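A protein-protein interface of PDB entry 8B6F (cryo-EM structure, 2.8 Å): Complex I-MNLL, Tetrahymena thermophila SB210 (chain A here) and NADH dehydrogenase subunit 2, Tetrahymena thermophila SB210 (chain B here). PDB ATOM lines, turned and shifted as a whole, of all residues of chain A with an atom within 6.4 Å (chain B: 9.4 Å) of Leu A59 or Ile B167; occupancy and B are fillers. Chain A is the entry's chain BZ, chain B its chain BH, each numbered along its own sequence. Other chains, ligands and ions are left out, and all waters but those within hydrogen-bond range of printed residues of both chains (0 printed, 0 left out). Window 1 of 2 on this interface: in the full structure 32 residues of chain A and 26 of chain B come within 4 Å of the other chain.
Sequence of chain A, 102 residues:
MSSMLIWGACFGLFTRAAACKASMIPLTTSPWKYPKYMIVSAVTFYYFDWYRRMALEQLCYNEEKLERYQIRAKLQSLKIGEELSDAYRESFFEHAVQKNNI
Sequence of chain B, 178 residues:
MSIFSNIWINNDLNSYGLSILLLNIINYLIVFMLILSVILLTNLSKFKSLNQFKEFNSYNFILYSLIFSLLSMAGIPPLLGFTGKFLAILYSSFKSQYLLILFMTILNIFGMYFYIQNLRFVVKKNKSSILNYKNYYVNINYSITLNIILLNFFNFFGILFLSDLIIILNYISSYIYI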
ATOM      1  N   ARG A  52     -12.619 -10.495  19.805  1.00  0.00           N
ATOM      2  CA  ARG A  52     -13.667  -9.781  20.528  1.00  0.00           C
ATOM      3  C   ARG A  52     -13.124  -9.169  21.810  1.00  0.00           C
ATOM      4  O   ARG A  52     -13.473  -8.037  22.161  1.00  0.00           O
ATOM      5  CB  ARG A  52     -14.845 -10.710  20.830  1.00  0.00           C
ATOM      6  CG  ARG A  52     -14.534 -11.872  21.760  1.00  0.00           C
ATOM      7  CD  ARG A  52     -15.808 -12.525  22.261  1.00  0.00           C
ATOM      8  NE  ARG A  52     -15.533 -13.548  23.261  1.00  0.00           N
ATOM      9  CZ  ARG A  52     -16.462 -14.172  23.971  1.00  0.00           C
ATOM     10  NH1 ARG A  52     -17.746 -13.889  23.829  1.00  0.00           N
ATOM     11  NH2 ARG A  52     -16.095 -15.100  24.848  1.00  0.00           N
ATOM     12  N   MET A  54      -9.926  -8.350  22.415  1.00  0.00           N
ATOM     13  CA  MET A  54      -9.049  -7.246  22.037  1.00  0.00           C
ATOM     14  C   MET A  54      -9.857  -6.012  21.666  1.00  0.00           C
ATOM     15  O   MET A  54      -9.507  -4.890  22.049  1.00  0.00           O
ATOM     16  CB  MET A  54      -8.146  -7.651  20.875  1.00  0.00           C
ATOM     17  CG  MET A  54      -6.856  -8.317  21.304  1.00  0.00           C
ATOM     18  SD  MET A  54      -5.632  -8.341  19.986  1.00  0.00           S
ATOM     19  CE  MET A  54      -5.230  -6.605  19.843  1.00  0.00           C
ATOM     20  N   ALA A  55     -10.936  -6.198  20.904  1.00  0.00           N
ATOM     21  CA  ALA A  55     -11.780  -5.071  20.529  1.00  0.00           C
ATOM     22  C   ALA A  55     -12.424  -4.438  21.755  1.00  0.00           C
ATOM     23  O   ALA A  55     -12.522  -3.211  21.850  1.00  0.00           O
ATOM     24  CB  ALA A  55     -12.851  -5.528  19.540  1.00  0.00           C
ATOM     25  N   LEU A  56     -12.870  -5.263  22.703  1.00  0.00           N
ATOM     26  CA  LEU A  56     -13.463  -4.731  23.923  1.00  0.00           C
ATOM     27  C   LEU A  56     -12.452  -3.917  24.717  1.00  0.00           C
ATOM     28  O   LEU A  56     -12.776  -2.836  25.223  1.00  0.00           O
ATOM     29  CB  LEU A  56     -14.015  -5.874  24.775  1.00  0.00           C
ATOM     30  CG  LEU A  56     -14.706  -5.477  26.081  1.00  0.00           C
ATOM     31  CD1 LEU A  56     -15.897  -4.573  25.817  1.00  0.00           C
ATOM     32  CD2 LEU A  56     -15.131  -6.715  26.846  1.00  0.00           C
ATOM     33  N   GLU A  57     -11.223  -4.415  24.840  1.00  0.00           N
ATOM     34  CA  GLU A  57     -10.199  -3.676  25.569  1.00  0.00           C
ATOM     35  C   GLU A  57      -9.901  -2.344  24.891  1.00  0.00           C
ATOM     36  O   GLU A  57      -9.812  -1.305  25.553  1.00  0.00           O
ATOM     37  CB  GLU A  57      -8.933  -4.524  25.682  1.00  0.00           C
ATOM     38  CG  GLU A  57      -7.819  -3.872  26.472  1.00  0.00           C
ATOM     39  CD  GLU A  57      -6.625  -4.788  26.642  1.00  0.00           C
ATOM     40  OE1 GLU A  57      -6.681  -5.932  26.145  1.00  0.00           O
ATOM     41  OE2 GLU A  57      -5.632  -4.367  27.270  1.00  0.00           O
ATOM     42  N   GLN A  58      -9.746  -2.355  23.567  1.00  0.00           N
ATOM     43  CA  GLN A  58      -9.454  -1.117  22.853  1.00  0.00           C
ATOM     44  C   GLN A  58     -10.633  -0.155  22.905  1.00  0.00           C
ATOM     45  O   GLN A  58     -10.437   1.063  22.945  1.00  0.00           O
ATOM     46  CB  GLN A  58      -9.073  -1.410  21.404  1.00  0.00           C
ATOM     47  CG  GLN A  58      -8.664  -0.173  20.618  1.00  0.00           C
ATOM     48  CD  GLN A  58      -7.541   0.596  21.280  1.00  0.00           C
ATOM     49  OE1 GLN A  58      -6.707   0.024  21.977  1.00  0.00           O
ATOM     50  NE2 GLN A  58      -7.523   1.908  21.073  1.00  0.00           N
ATOM     51  N   LEU A  59     -11.856  -0.683  22.905  1.00  0.00           N
ATOM     52  CA  LEU A  59     -13.028   0.171  23.057  1.00  0.00           C
ATOM     53  C   LEU A  59     -13.056   0.821  24.430  1.00  0.00           C
ATOM     54  O   LEU A  59     -13.369   2.010  24.552  1.00  0.00           O
ATOM     55  CB  LEU A  59     -14.297  -0.643  22.819  1.00  0.00           C
ATOM     56  CG  LEU A  59     -15.625   0.013  23.199  1.00  0.00           C
ATOM     57  CD1 LEU A  59     -15.801   1.358  22.512  1.00  0.00           C
ATOM     58  CD2 LEU A  59     -16.765  -0.918  22.842  1.00  0.00           C
ATOM     59  N   CYS A  60     -12.720   0.066  25.475  1.00  0.00           N
ATOM     60  CA  CYS A  60     -12.648   0.653  26.807  1.00  0.00           C
ATOM     61  C   CYS A  60     -11.612   1.767  26.857  1.00  0.00           C
ATOM     62  O   CYS A  60     -11.839   2.810  27.482  1.00  0.00           O
ATOM     63  CB  CYS A  60     -12.323  -0.427  27.837  1.00  0.00           C
ATOM     64  SG  CYS A  60     -13.681  -1.570  28.164  1.00  0.00           S
ATOM     65  N   TYR A  61     -10.461   1.564  26.215  1.00  0.00           N
ATOM     66  CA  TYR A  61      -9.446   2.611  26.172  1.00  0.00           C
ATOM     67  C   TYR A  61      -9.923   3.811  25.363  1.00  0.00           C
ATOM     68  O   TYR A  61      -9.659   4.960  25.735  1.00  0.00           O
ATOM     69  CB  TYR A  61      -8.146   2.054  25.595  1.00  0.00           C
ATOM     70  CG  TYR A  61      -7.341   1.259  26.596  1.00  0.00           C
ATOM     71  CD1 TYR A  61      -6.645   1.890  27.617  1.00  0.00           C
ATOM     72  CD2 TYR A  61      -7.277  -0.124  26.517  1.00  0.00           C
ATOM     73  CE1 TYR A  61      -5.910   1.165  28.533  1.00  0.00           C
ATOM     74  CE2 TYR A  61      -6.546  -0.857  27.426  1.00  0.00           C
ATOM     75  CZ  TYR A  61      -5.864  -0.209  28.431  1.00  0.00           C
ATOM     76  OH  TYR A  61      -5.135  -0.941  29.336  1.00  0.00           O
ATOM     77  N   ASN A  62     -10.617   3.569  24.248  1.00  0.00           N
ATOM     78  CA  ASN A  62     -11.097   4.677  23.429  1.00  0.00           C
ATOM     79  C   ASN A  62     -12.143   5.506  24.159  1.00  0.00           C
ATOM     80  O   ASN A  62     -12.230   6.720  23.941  1.00  0.00           O
ATOM     81  CB  ASN A  62     -11.685   4.154  22.119  1.00  0.00           C
ATOM     82  CG  ASN A  62     -10.636   3.584  21.195  1.00  0.00           C
ATOM     83  OD1 ASN A  62      -9.447   3.867  21.335  1.00  0.00           O
ATOM     84  ND2 ASN A  62     -11.073   2.781  20.232  1.00  0.00           N
ATOM     85  N   GLU A  63     -12.944   4.877  25.018  1.00  0.00           N
ATOM     86  CA  GLU A  63     -13.961   5.620  25.751  1.00  0.00           C
ATOM     87  C   GLU A  63     -13.342   6.668  26.663  1.00  0.00           C
ATOM     88  O   GLU A  63     -13.971   7.694  26.943  1.00  0.00           O
ATOM     89  CB  GLU A  63     -14.830   4.655  26.553  1.00  0.00           C
ATOM     90  CG  GLU A  63     -15.785   3.863  25.683  1.00  0.00           C
ATOM     91  CD  GLU A  63     -16.614   2.879  26.474  1.00  0.00           C
ATOM     92  OE1 GLU A  63     -16.412   2.783  27.701  1.00  0.00           O
ATOM     93  OE2 GLU A  63     -17.467   2.200  25.868  1.00  0.00           O
ATOM     94  N   GLU A  64     -12.117   6.436  27.138  1.00  0.00           N
ATOM     95  CA  GLU A  64     -11.433   7.452  27.930  1.00  0.00           C
ATOM     96  C   GLU A  64     -11.221   8.721  27.116  1.00  0.00           C
ATOM     97  O   GLU A  64     -11.492   9.830  27.587  1.00  0.00           O
ATOM     98  CB  GLU A  64     -10.098   6.911  28.439  1.00  0.00           C
ATOM     99  CG  GLU A  64     -10.235   5.751  29.402  1.00  0.00           C
ATOM    100  CD  GLU A  64      -8.895   5.212  29.857  1.00  0.00           C
ATOM    101  OE1 GLU A  64      -7.880   5.488  29.186  1.00  0.00           O
ATOM    102  OE2 GLU A  64      -8.857   4.516  30.892  1.00  0.00           O
ATOM    103  N   LEU B  13     -22.889   7.035  25.984  1.00  0.00           N
ATOM    104  CA  LEU B  13     -21.879   6.745  24.973  1.00  0.00           C
ATOM    105  C   LEU B  13     -22.363   7.334  23.655  1.00  0.00           C
ATOM    106  O   LEU B  13     -23.312   6.825  23.050  1.00  0.00           O
ATOM    107  CB  LEU B  13     -21.643   5.240  24.858  1.00  0.00           C
ATOM    108  CG  LEU B  13     -20.539   4.789  23.899  1.00  0.00           C
ATOM    109  CD1 LEU B  13     -19.179   5.261  24.382  1.00  0.00           C
ATOM    110  CD2 LEU B  13     -20.560   3.280  23.743  1.00  0.00           C
ATOM    111  N   ASN B  14     -21.712   8.411  23.210  1.00  0.00           N
ATOM    112  CA  ASN B  14     -22.184   9.118  22.026  1.00  0.00           C
ATOM    113  C   ASN B  14     -22.085   8.246  20.781  1.00  0.00           C
ATOM    114  O   ASN B  14     -22.968   8.284  19.917  1.00  0.00           O
ATOM    115  CB  ASN B  14     -21.385  10.408  21.840  1.00  0.00           C
ATOM    116  CG  ASN B  14     -22.044  11.362  20.871  1.00  0.00           C
ATOM    117  OD1 ASN B  14     -23.128  11.092  20.358  1.00  0.00           O
ATOM    118  ND2 ASN B  14     -21.397  12.493  20.624  1.00  0.00           N
ATOM    119  N   SER B  15     -21.018   7.458  20.671  1.00  0.00           N
ATOM    120  CA  SER B  15     -20.798   6.605  19.504  1.00  0.00           C
ATOM    121  C   SER B  15     -21.544   5.278  19.667  1.00  0.00           C
ATOM    122  O   SER B  15     -20.963   4.194  19.664  1.00  0.00           O
ATOM    123  CB  SER B  15     -19.308   6.373  19.306  1.00  0.00           C
ATOM    124  OG  SER B  15     -18.766   5.701  20.430  1.00  0.00           O
ATOM    125  N   TYR B  16     -22.858   5.385  19.808  1.00  0.00           N
ATOM    126  CA  TYR B  16     -23.731   4.226  19.939  1.00  0.00           C
ATOM    127  C   TYR B  16     -24.818   4.186  18.881  1.00  0.00           C
ATOM    128  O   TYR B  16     -25.154   3.107  18.391  1.00  0.00           O
ATOM    129  CB  TYR B  16     -24.375   4.204  21.333  1.00  0.00           C
ATOM    130  CG  TYR B  16     -25.080   2.906  21.649  1.00  0.00           C
ATOM    131  CD1 TYR B  16     -26.422   2.729  21.338  1.00  0.00           C
ATOM    132  CD2 TYR B  16     -24.405   1.857  22.255  1.00  0.00           C
ATOM    133  CE1 TYR B  16     -27.071   1.543  21.622  1.00  0.00           C
ATOM    134  CE2 TYR B  16     -25.043   0.667  22.542  1.00  0.00           C
ATOM    135  CZ  TYR B  16     -26.376   0.517  22.223  1.00  0.00           C
ATOM    136  OH  TYR B  16     -27.015  -0.666  22.508  1.00  0.00           O
ATOM    137  N   SER B  19     -23.265   2.844  15.768  1.00  0.00           N
ATOM    138  CA  SER B  19     -23.102   1.398  15.857  1.00  0.00           C
ATOM    139  C   SER B  19     -24.422   0.682  15.606  1.00  0.00           C
ATOM    140  O   SER B  19     -24.455  -0.361  14.943  1.00  0.00           O
ATOM    141  CB  SER B  19     -22.536   1.016  17.224  1.00  0.00           C
ATOM    142  OG  SER B  19     -23.487   1.241  18.249  1.00  0.00           O
ATOM    143  N   ILE B  20     -25.522   1.219  16.137  1.00  0.00           N
ATOM    144  CA  ILE B  20     -26.829   0.611  15.905  1.00  0.00           C
ATOM    145  C   ILE B  20     -27.192   0.683  14.428  1.00  0.00           C
ATOM    146  O   ILE B  20     -27.745  -0.268  13.863  1.00  0.00           O
ATOM    147  CB  ILE B  20     -27.898   1.285  16.787  1.00  0.00           C
ATOM    148  CG1 ILE B  20     -27.637   1.013  18.275  1.00  0.00           C
ATOM    149  CG2 ILE B  20     -29.296   0.807  16.403  1.00  0.00           C
ATOM    150  CD1 ILE B  20     -27.603  -0.451  18.664  1.00  0.00           C
ATOM    151  N   LEU B  23     -25.267  -1.913  12.683  1.00  0.00           N
ATOM    152  CA  LEU B  23     -25.843  -3.218  12.981  1.00  0.00           C
ATOM    153  C   LEU B  23     -27.079  -3.480  12.132  1.00  0.00           C
ATOM    154  O   LEU B  23     -27.257  -4.585  11.607  1.00  0.00           O
ATOM    155  CB  LEU B  23     -26.186  -3.306  14.468  1.00  0.00           C
ATOM    156  CG  LEU B  23     -26.770  -4.635  14.943  1.00  0.00           C
ATOM    157  CD1 LEU B  23     -25.772  -5.765  14.749  1.00  0.00           C
ATOM    158  CD2 LEU B  23     -27.177  -4.527  16.393  1.00  0.00           C
ATOM    159  N   LEU B  87     -33.406  -2.803  18.577  1.00  0.00           N
ATOM    160  CA  LEU B  87     -32.358  -1.884  19.004  1.00  0.00           C
ATOM    161  C   LEU B  87     -32.583  -0.479  18.465  1.00  0.00           C
ATOM    162  O   LEU B  87     -32.251   0.500  19.143  1.00  0.00           O
ATOM    163  CB  LEU B  87     -30.996  -2.418  18.576  1.00  0.00           C
ATOM    164  CG  LEU B  87     -30.515  -3.629  19.378  1.00  0.00           C
ATOM    165  CD1 LEU B  87     -29.301  -4.255  18.732  1.00  0.00           C
ATOM    166  CD2 LEU B  87     -30.207  -3.244  20.817  1.00  0.00           C
ATOM    167  N   PHE B 161     -25.498 -14.355  20.156  1.00  0.00           N
ATOM    168  CA  PHE B 161     -24.162 -13.839  19.899  1.00  0.00           C
ATOM    169  C   PHE B 161     -24.158 -12.356  19.550  1.00  0.00           C
ATOM    170  O   PHE B 161     -23.116 -11.828  19.156  1.00  0.00           O
ATOM    171  CB  PHE B 161     -23.510 -14.636  18.769  1.00  0.00           C
ATOM    172  CG  PHE B 161     -23.619 -16.119  18.942  1.00  0.00           C
ATOM    173  CD1 PHE B 161     -22.667 -16.815  19.665  1.00  0.00           C
ATOM    174  CD2 PHE B 161     -24.677 -16.816  18.388  1.00  0.00           C
ATOM    175  CE1 PHE B 161     -22.766 -18.179  19.830  1.00  0.00           C
ATOM    176  CE2 PHE B 161     -24.783 -18.182  18.549  1.00  0.00           C
ATOM    177  CZ  PHE B 161     -23.825 -18.864  19.271  1.00  0.00           C
ATOM    178  N   LEU B 162     -25.294 -11.671  19.694  1.00  0.00           N
ATOM    179  CA  LEU B 162     -25.369 -10.277  19.274  1.00  0.00           C
ATOM    180  C   LEU B 162     -24.483  -9.378  20.126  1.00  0.00           C
ATOM    181  O   LEU B 162     -24.036  -8.327  19.654  1.00  0.00           O
ATOM    182  CB  LEU B 162     -26.816  -9.790  19.331  1.00  0.00           C
ATOM    183  CG  LEU B 162     -27.108  -8.451  18.651  1.00  0.00           C
ATOM    184  CD1 LEU B 162     -26.923  -8.550  17.148  1.00  0.00           C
ATOM    185  CD2 LEU B 162     -28.510  -7.982  18.987  1.00  0.00           C
ATOM    186  N   SER B 163     -24.217  -9.765  21.375  1.00  0.00           N
ATOM    187  CA  SER B 163     -23.406  -8.924  22.250  1.00  0.00           C
ATOM    188  C   SER B 163     -22.008  -8.726  21.680  1.00  0.00           C
ATOM    189  O   SER B 163     -21.456  -7.622  21.739  1.00  0.00           O
ATOM    190  CB  SER B 163     -23.337  -9.530  23.652  1.00  0.00           C
ATOM    191  OG  SER B 163     -22.794 -10.837  23.623  1.00  0.00           O
ATOM    192  N   ASP B 164     -21.415  -9.785  21.128  1.00  0.00           N
ATOM    193  CA  ASP B 164     -20.088  -9.660  20.532  1.00  0.00           C
ATOM    194  C   ASP B 164     -20.112  -8.749  19.313  1.00  0.00           C
ATOM    195  O   ASP B 164     -19.224  -7.908  19.142  1.00  0.00           O
ATOM    196  CB  ASP B 164     -19.554 -11.039  20.154  1.00  0.00           C
ATOM    197  CG  ASP B 164     -19.604 -12.012  21.306  1.00  0.00           C
ATOM    198  OD1 ASP B 164     -19.288 -11.608  22.445  1.00  0.00           O
ATOM    199  OD2 ASP B 164     -19.970 -13.182  21.075  1.00  0.00           O
ATOM    200  N   LEU B 165     -21.120  -8.902  18.452  1.00  0.00           N
ATOM    201  CA  LEU B 165     -21.221  -8.036  17.284  1.00  0.00           C
ATOM    202  C   LEU B 165     -21.440  -6.587  17.697  1.00  0.00           C
ATOM    203  O   LEU B 165     -20.872  -5.669  17.096  1.00  0.00           O
ATOM    204  CB  LEU B 165     -22.349  -8.518  16.372  1.00  0.00           C
ATOM    205  CG  LEU B 165     -22.560  -7.725  15.079  1.00  0.00           C
ATOM    206  CD1 LEU B 165     -21.292  -7.689  14.241  1.00  0.00           C
ATOM    207  CD2 LEU B 165     -23.706  -8.317  14.276  1.00  0.00           C
ATOM    208  N   ILE B 166     -22.261  -6.361  18.723  1.00  0.00           N
ATOM    209  CA  ILE B 166     -22.476  -5.004  19.217  1.00  0.00           C
ATOM    210  C   ILE B 166     -21.176  -4.431  19.768  1.00  0.00           C
ATOM    211  O   ILE B 166     -20.865  -3.252  19.564  1.00  0.00           O
ATOM    212  CB  ILE B 166     -23.601  -4.992  20.268  1.00  0.00           C
ATOM    213  CG1 ILE B 166     -24.943  -5.280  19.591  1.00  0.00           C
ATOM    214  CG2 ILE B 166     -23.648  -3.651  21.000  1.00  0.00           C
ATOM    215  CD1 ILE B 166     -26.096  -5.450  20.550  1.00  0.00           C
ATOM    216  N   ILE B 167     -20.407  -5.245  20.493  1.00  0.00           N
ATOM    217  CA  ILE B 167     -19.126  -4.777  21.015  1.00  0.00           C
ATOM    218  C   ILE B 167     -18.206  -4.377  19.869  1.00  0.00           C
ATOM    219  O   ILE B 167     -17.552  -3.331  19.910  1.00  0.00           O
ATOM    220  CB  ILE B 167     -18.483  -5.861  21.901  1.00  0.00           C
ATOM    221  CG1 ILE B 167     -19.242  -5.992  23.222  1.00  0.00           C
ATOM    222  CG2 ILE B 167     -17.012  -5.544  22.171  1.00  0.00           C
ATOM    223  CD1 ILE B 167     -18.880  -7.233  24.014  1.00  0.00           C
ATOM    224  N   ILE B 168     -18.140  -5.210  18.829  1.00  0.00           N
ATOM    225  CA  ILE B 168     -17.248  -4.919  17.712  1.00  0.00           C
ATOM    226  C   ILE B 168     -17.689  -3.655  16.986  1.00  0.00           C
ATOM    227  O   ILE B 168     -16.861  -2.806  16.634  1.00  0.00           O
ATOM    228  CB  ILE B 168     -17.180  -6.129  16.762  1.00  0.00           C
ATOM    229  CG1 ILE B 168     -16.468  -7.295  17.453  1.00  0.00           C
ATOM    230  CG2 ILE B 168     -16.465  -5.764  15.464  1.00  0.00           C
ATOM    231  CD1 ILE B 168     -16.522  -8.601  16.689  1.00  0.00           C
ATOM    232  N   LEU B 169     -18.992  -3.504  16.748  1.00  0.00           N
ATOM    233  CA  LEU B 169     -19.476  -2.316  16.051  1.00  0.00           C
ATOM    234  C   LEU B 169     -19.246  -1.055  16.873  1.00  0.00           C
ATOM    235  O   LEU B 169     -18.873  -0.011  16.325  1.00  0.00           O
ATOM    236  CB  LEU B 169     -20.955  -2.477  15.709  1.00  0.00           C
ATOM    237  CG  LEU B 169     -21.271  -3.558  14.671  1.00  0.00           C
ATOM    238  CD1 LEU B 169     -22.769  -3.704  14.501  1.00  0.00           C
ATOM    239  CD2 LEU B 169     -20.617  -3.246  13.335  1.00  0.00           C
ATOM    240  N   ASN B 170     -19.470  -1.124  18.185  1.00  0.00           N
ATOM    241  CA  ASN B 170     -19.191   0.025  19.039  1.00  0.00           C
ATOM    242  C   ASN B 170     -17.703   0.342  19.060  1.00  0.00           C
ATOM    243  O   ASN B 170     -17.307   1.511  19.095  1.00  0.00           O
ATOM    244  CB  ASN B 170     -19.701  -0.234  20.455  1.00  0.00           C
ATOM    245  CG  ASN B 170     -21.190  -0.015  20.579  1.00  0.00           C
ATOM    246  OD1 ASN B 170     -21.636   1.056  20.984  1.00  0.00           O
ATOM    247  ND2 ASN B 170     -21.972  -1.029  20.227  1.00  0.00           N
ATOM    248  N   TYR B 171     -16.866  -0.692  19.051  1.00  0.00           N
ATOM    249  CA  TYR B 171     -15.428  -0.479  18.975  1.00  0.00           C
ATOM    250  C   TYR B 171     -15.047   0.237  17.686  1.00  0.00           C
ATOM    251  O   TYR B 171     -14.212   1.149  17.696  1.00  0.00           O
ATOM    252  CB  TYR B 171     -14.715  -1.822  19.092  1.00  0.00           C
ATOM    253  CG  TYR B 171     -13.361  -1.874  18.449  1.00  0.00           C
ATOM    254  CD1 TYR B 171     -12.258  -1.327  19.080  1.00  0.00           C
ATOM    255  CD2 TYR B 171     -13.178  -2.498  17.225  1.00  0.00           C
ATOM    256  CE1 TYR B 171     -11.017  -1.382  18.508  1.00  0.00           C
ATOM    257  CE2 TYR B 171     -11.938  -2.558  16.643  1.00  0.00           C
ATOM    258  CZ  TYR B 171     -10.861  -2.004  17.295  1.00  0.00           C
ATOM    259  OH  TYR B 171      -9.623  -2.061  16.716  1.00  0.00           O
ATOM    260  N   ILE B 172     -15.645  -0.165  16.563  1.00  0.00           N
ATOM    261  CA  ILE B 172     -15.356   0.482  15.286  1.00  0.00           C
ATOM    262  C   ILE B 172     -15.817   1.933  15.306  1.00  0.00           C
ATOM    263  O   ILE B 172     -15.111   2.832  14.835  1.00  0.00           O
ATOM    264  CB  ILE B 172     -16.006  -0.305  14.133  1.00  0.00           C
ATOM    265  CG1 ILE B 172     -15.319  -1.664  13.975  1.00  0.00           C
ATOM    266  CG2 ILE B 172     -15.944   0.486  12.828  1.00  0.00           C
ATOM    267  CD1 ILE B 172     -16.019  -2.604  13.021  1.00  0.00           C
ATOM    268  N   SER B 173     -17.011   2.184  15.842  1.00  0.00           N
ATOM    269  CA  SER B 173     -17.571   3.531  15.799  1.00  0.00           C
ATOM    270  C   SER B 173     -16.893   4.460  16.798  1.00  0.00           C
ATOM    271  O   SER B 173     -16.880   5.677  16.591  1.00  0.00           O
ATOM    272  CB  SER B 173     -19.076   3.483  16.057  1.00  0.00           C
ATOM    273  OG  SER B 173     -19.358   3.002  17.358  1.00  0.00           O
ATOM    274  N   SER B 174     -16.325   3.918  17.876  1.00  0.00           N
ATOM    275  CA  SER B 174     -15.715   4.773  18.888  1.00  0.00           C
ATOM    276  C   SER B 174     -14.544   5.567  18.332  1.00  0.00           C
ATOM    277  O   SER B 174     -14.206   6.616  18.888  1.00  0.00           O
ATOM    278  CB  SER B 174     -15.257   3.939  20.083  1.00  0.00           C
ATOM    279  OG  SER B 174     -14.255   3.011  19.709  1.00  0.00           O
ATOM    280  N   TYR B 175     -13.916   5.097  17.255  1.00  0.00           N
ATOM    281  CA  TYR B 175     -12.826   5.857  16.657  1.00  0.00           C
ATOM    282  C   TYR B 175     -13.319   7.185  16.109  1.00  0.00           C
ATOM    283  O   TYR B 175     -12.589   8.182  16.144  1.00  0.00           O
ATOM    284  CB  TYR B 175     -12.153   5.045  15.554  1.00  0.00           C
ATOM    285  CG  TYR B 175     -11.332   3.894  16.074  1.00  0.00           C
ATOM    286  CD1 TYR B 175     -10.191   4.124  16.828  1.00  0.00           C
ATOM    287  CD2 TYR B 175     -11.687   2.582  15.804  1.00  0.00           C
ATOM    288  CE1 TYR B 175      -9.430   3.084  17.305  1.00  0.00           C
ATOM    289  CE2 TYR B 175     -10.931   1.531  16.277  1.00  0.00           C
ATOM    290  CZ  TYR B 175      -9.802   1.790  17.024  1.00  0.00           C
ATOM    291  OH  TYR B 175      -9.042   0.750  17.499  1.00  0.00           O
ATOM    292  N   ILE B 176     -14.547   7.219  15.598  1.00  0.00           N
ATOM    293  CA  ILE B 176     -15.138   8.474  15.159  1.00  0.00           C
ATOM    294  C   ILE B 176     -15.334   9.358  16.384  1.00  0.00           C
ATOM    295  O   ILE B 176     -15.919   8.933  17.389  1.00  0.00           O
ATOM    296  CB  ILE B 176     -16.455   8.204  14.413  1.00  0.00           C
ATOM    297  CG1 ILE B 176     -16.561   9.101  13.181  1.00  0.00           C
ATOM    298  CG2 ILE B 176     -17.676   8.425  15.313  1.00  0.00           C
ATOM    299  CD1 ILE B 176     -17.745   8.761  12.296  1.00  0.00           C
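The guanidinium group (NH1) of Arg A52 lies within salt-bridge range of the side-chain carboxylate (OD1) of Asp B164 (3.1 Å).
OG of Ser B174 sits at hydrogen-bond distance from ND2 of Asn A62.
Of the 12 printed residues of chain A, 7 touch a printed residue of chain B.
Along chain A the printed residues that touch a printed residue of chain B span positions 52 to 63.
Among the printed residues, 12 pairs touch across the chains.
Among the printed residues, Asp or Glu carboxylates within 4 Å of a Lys or Arg side-chain nitrogen of the other chain: Arg A52 with Asp B164.
Leu A59 touches four residues of chain B.
No residue of chain B comes within 4 Å of Cys A60.
Printed residues of chain A within 4 Å of Tyr B171: Ala A55 (3.4 Å), Gln A58 (3.4 Å) and Leu A59 (3.8 Å).
Of the printed residues of chain A, Tyr B175 touches Gln A58 and Asn A62.
Printed residues of chain B within 4 Å of Arg A52: Asp B164.
Of the printed residues of chain B, Gln A58 touches Tyr B171 (3.4 Å) and Tyr B175 (3.3 Å).
Leu B165 touches none of the printed residues of chain A.
The nearest residue of chain A that does not touch Ile B167 is Arg A52 (4.3 Å).
O of Ala A55 touches CD1 of Tyr B171 (3.4 Å).
CD1 of Leu A56 touches CG2 of Ile B167 (3.9 Å).
CG of Gln A58 touches CE1 of Tyr B171, 3.4 Å away.
Gln A58 touches Tyr B175.
Ile B167 touches Leu A59 (O to CD2, 3.9 Å).
Leu A59 touches Asn B170.
Tyr B171 touches Leu A59 (N to CD2, 3.8 Å).
Leu A59 touches Ser B174.
Asn A62 touches Tyr B175 (ND2 to CE1, 3.4 Å).
Glu A63 touches Leu B13 (OE2 to CD1, 3.8 Å).
The backbone carbonyl oxygen (O) of Ile B166 lies within hydrogen-bond range of the side-chain amide nitrogen (ND2) of Asn B170 (2.6 Å).
NE2 of Gln A58 lies within hydrogen-bond range of OD1 of Asn A62, 2.8 Å away.
The backbone carbonyl oxygen of Ser B15 sits close to the side-chain amide oxygen of Asn B170, at 3.5 Å.
The backbone carbonyl oxygen (O) of Tyr B171 lies within hydrogen-bond range of the side-chain hydroxyl (OG) of Ser B174, 2.7 Å away.
OH of Tyr B171 sits at hydrogen-bond distance from OH of Tyr B175 (3.0 Å).
The backbone carbonyl oxygen (O) of Leu A56 lies within hydrogen-bond range of the side-chain sulfur (SG) of Cys A60, 3.3 Å away.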
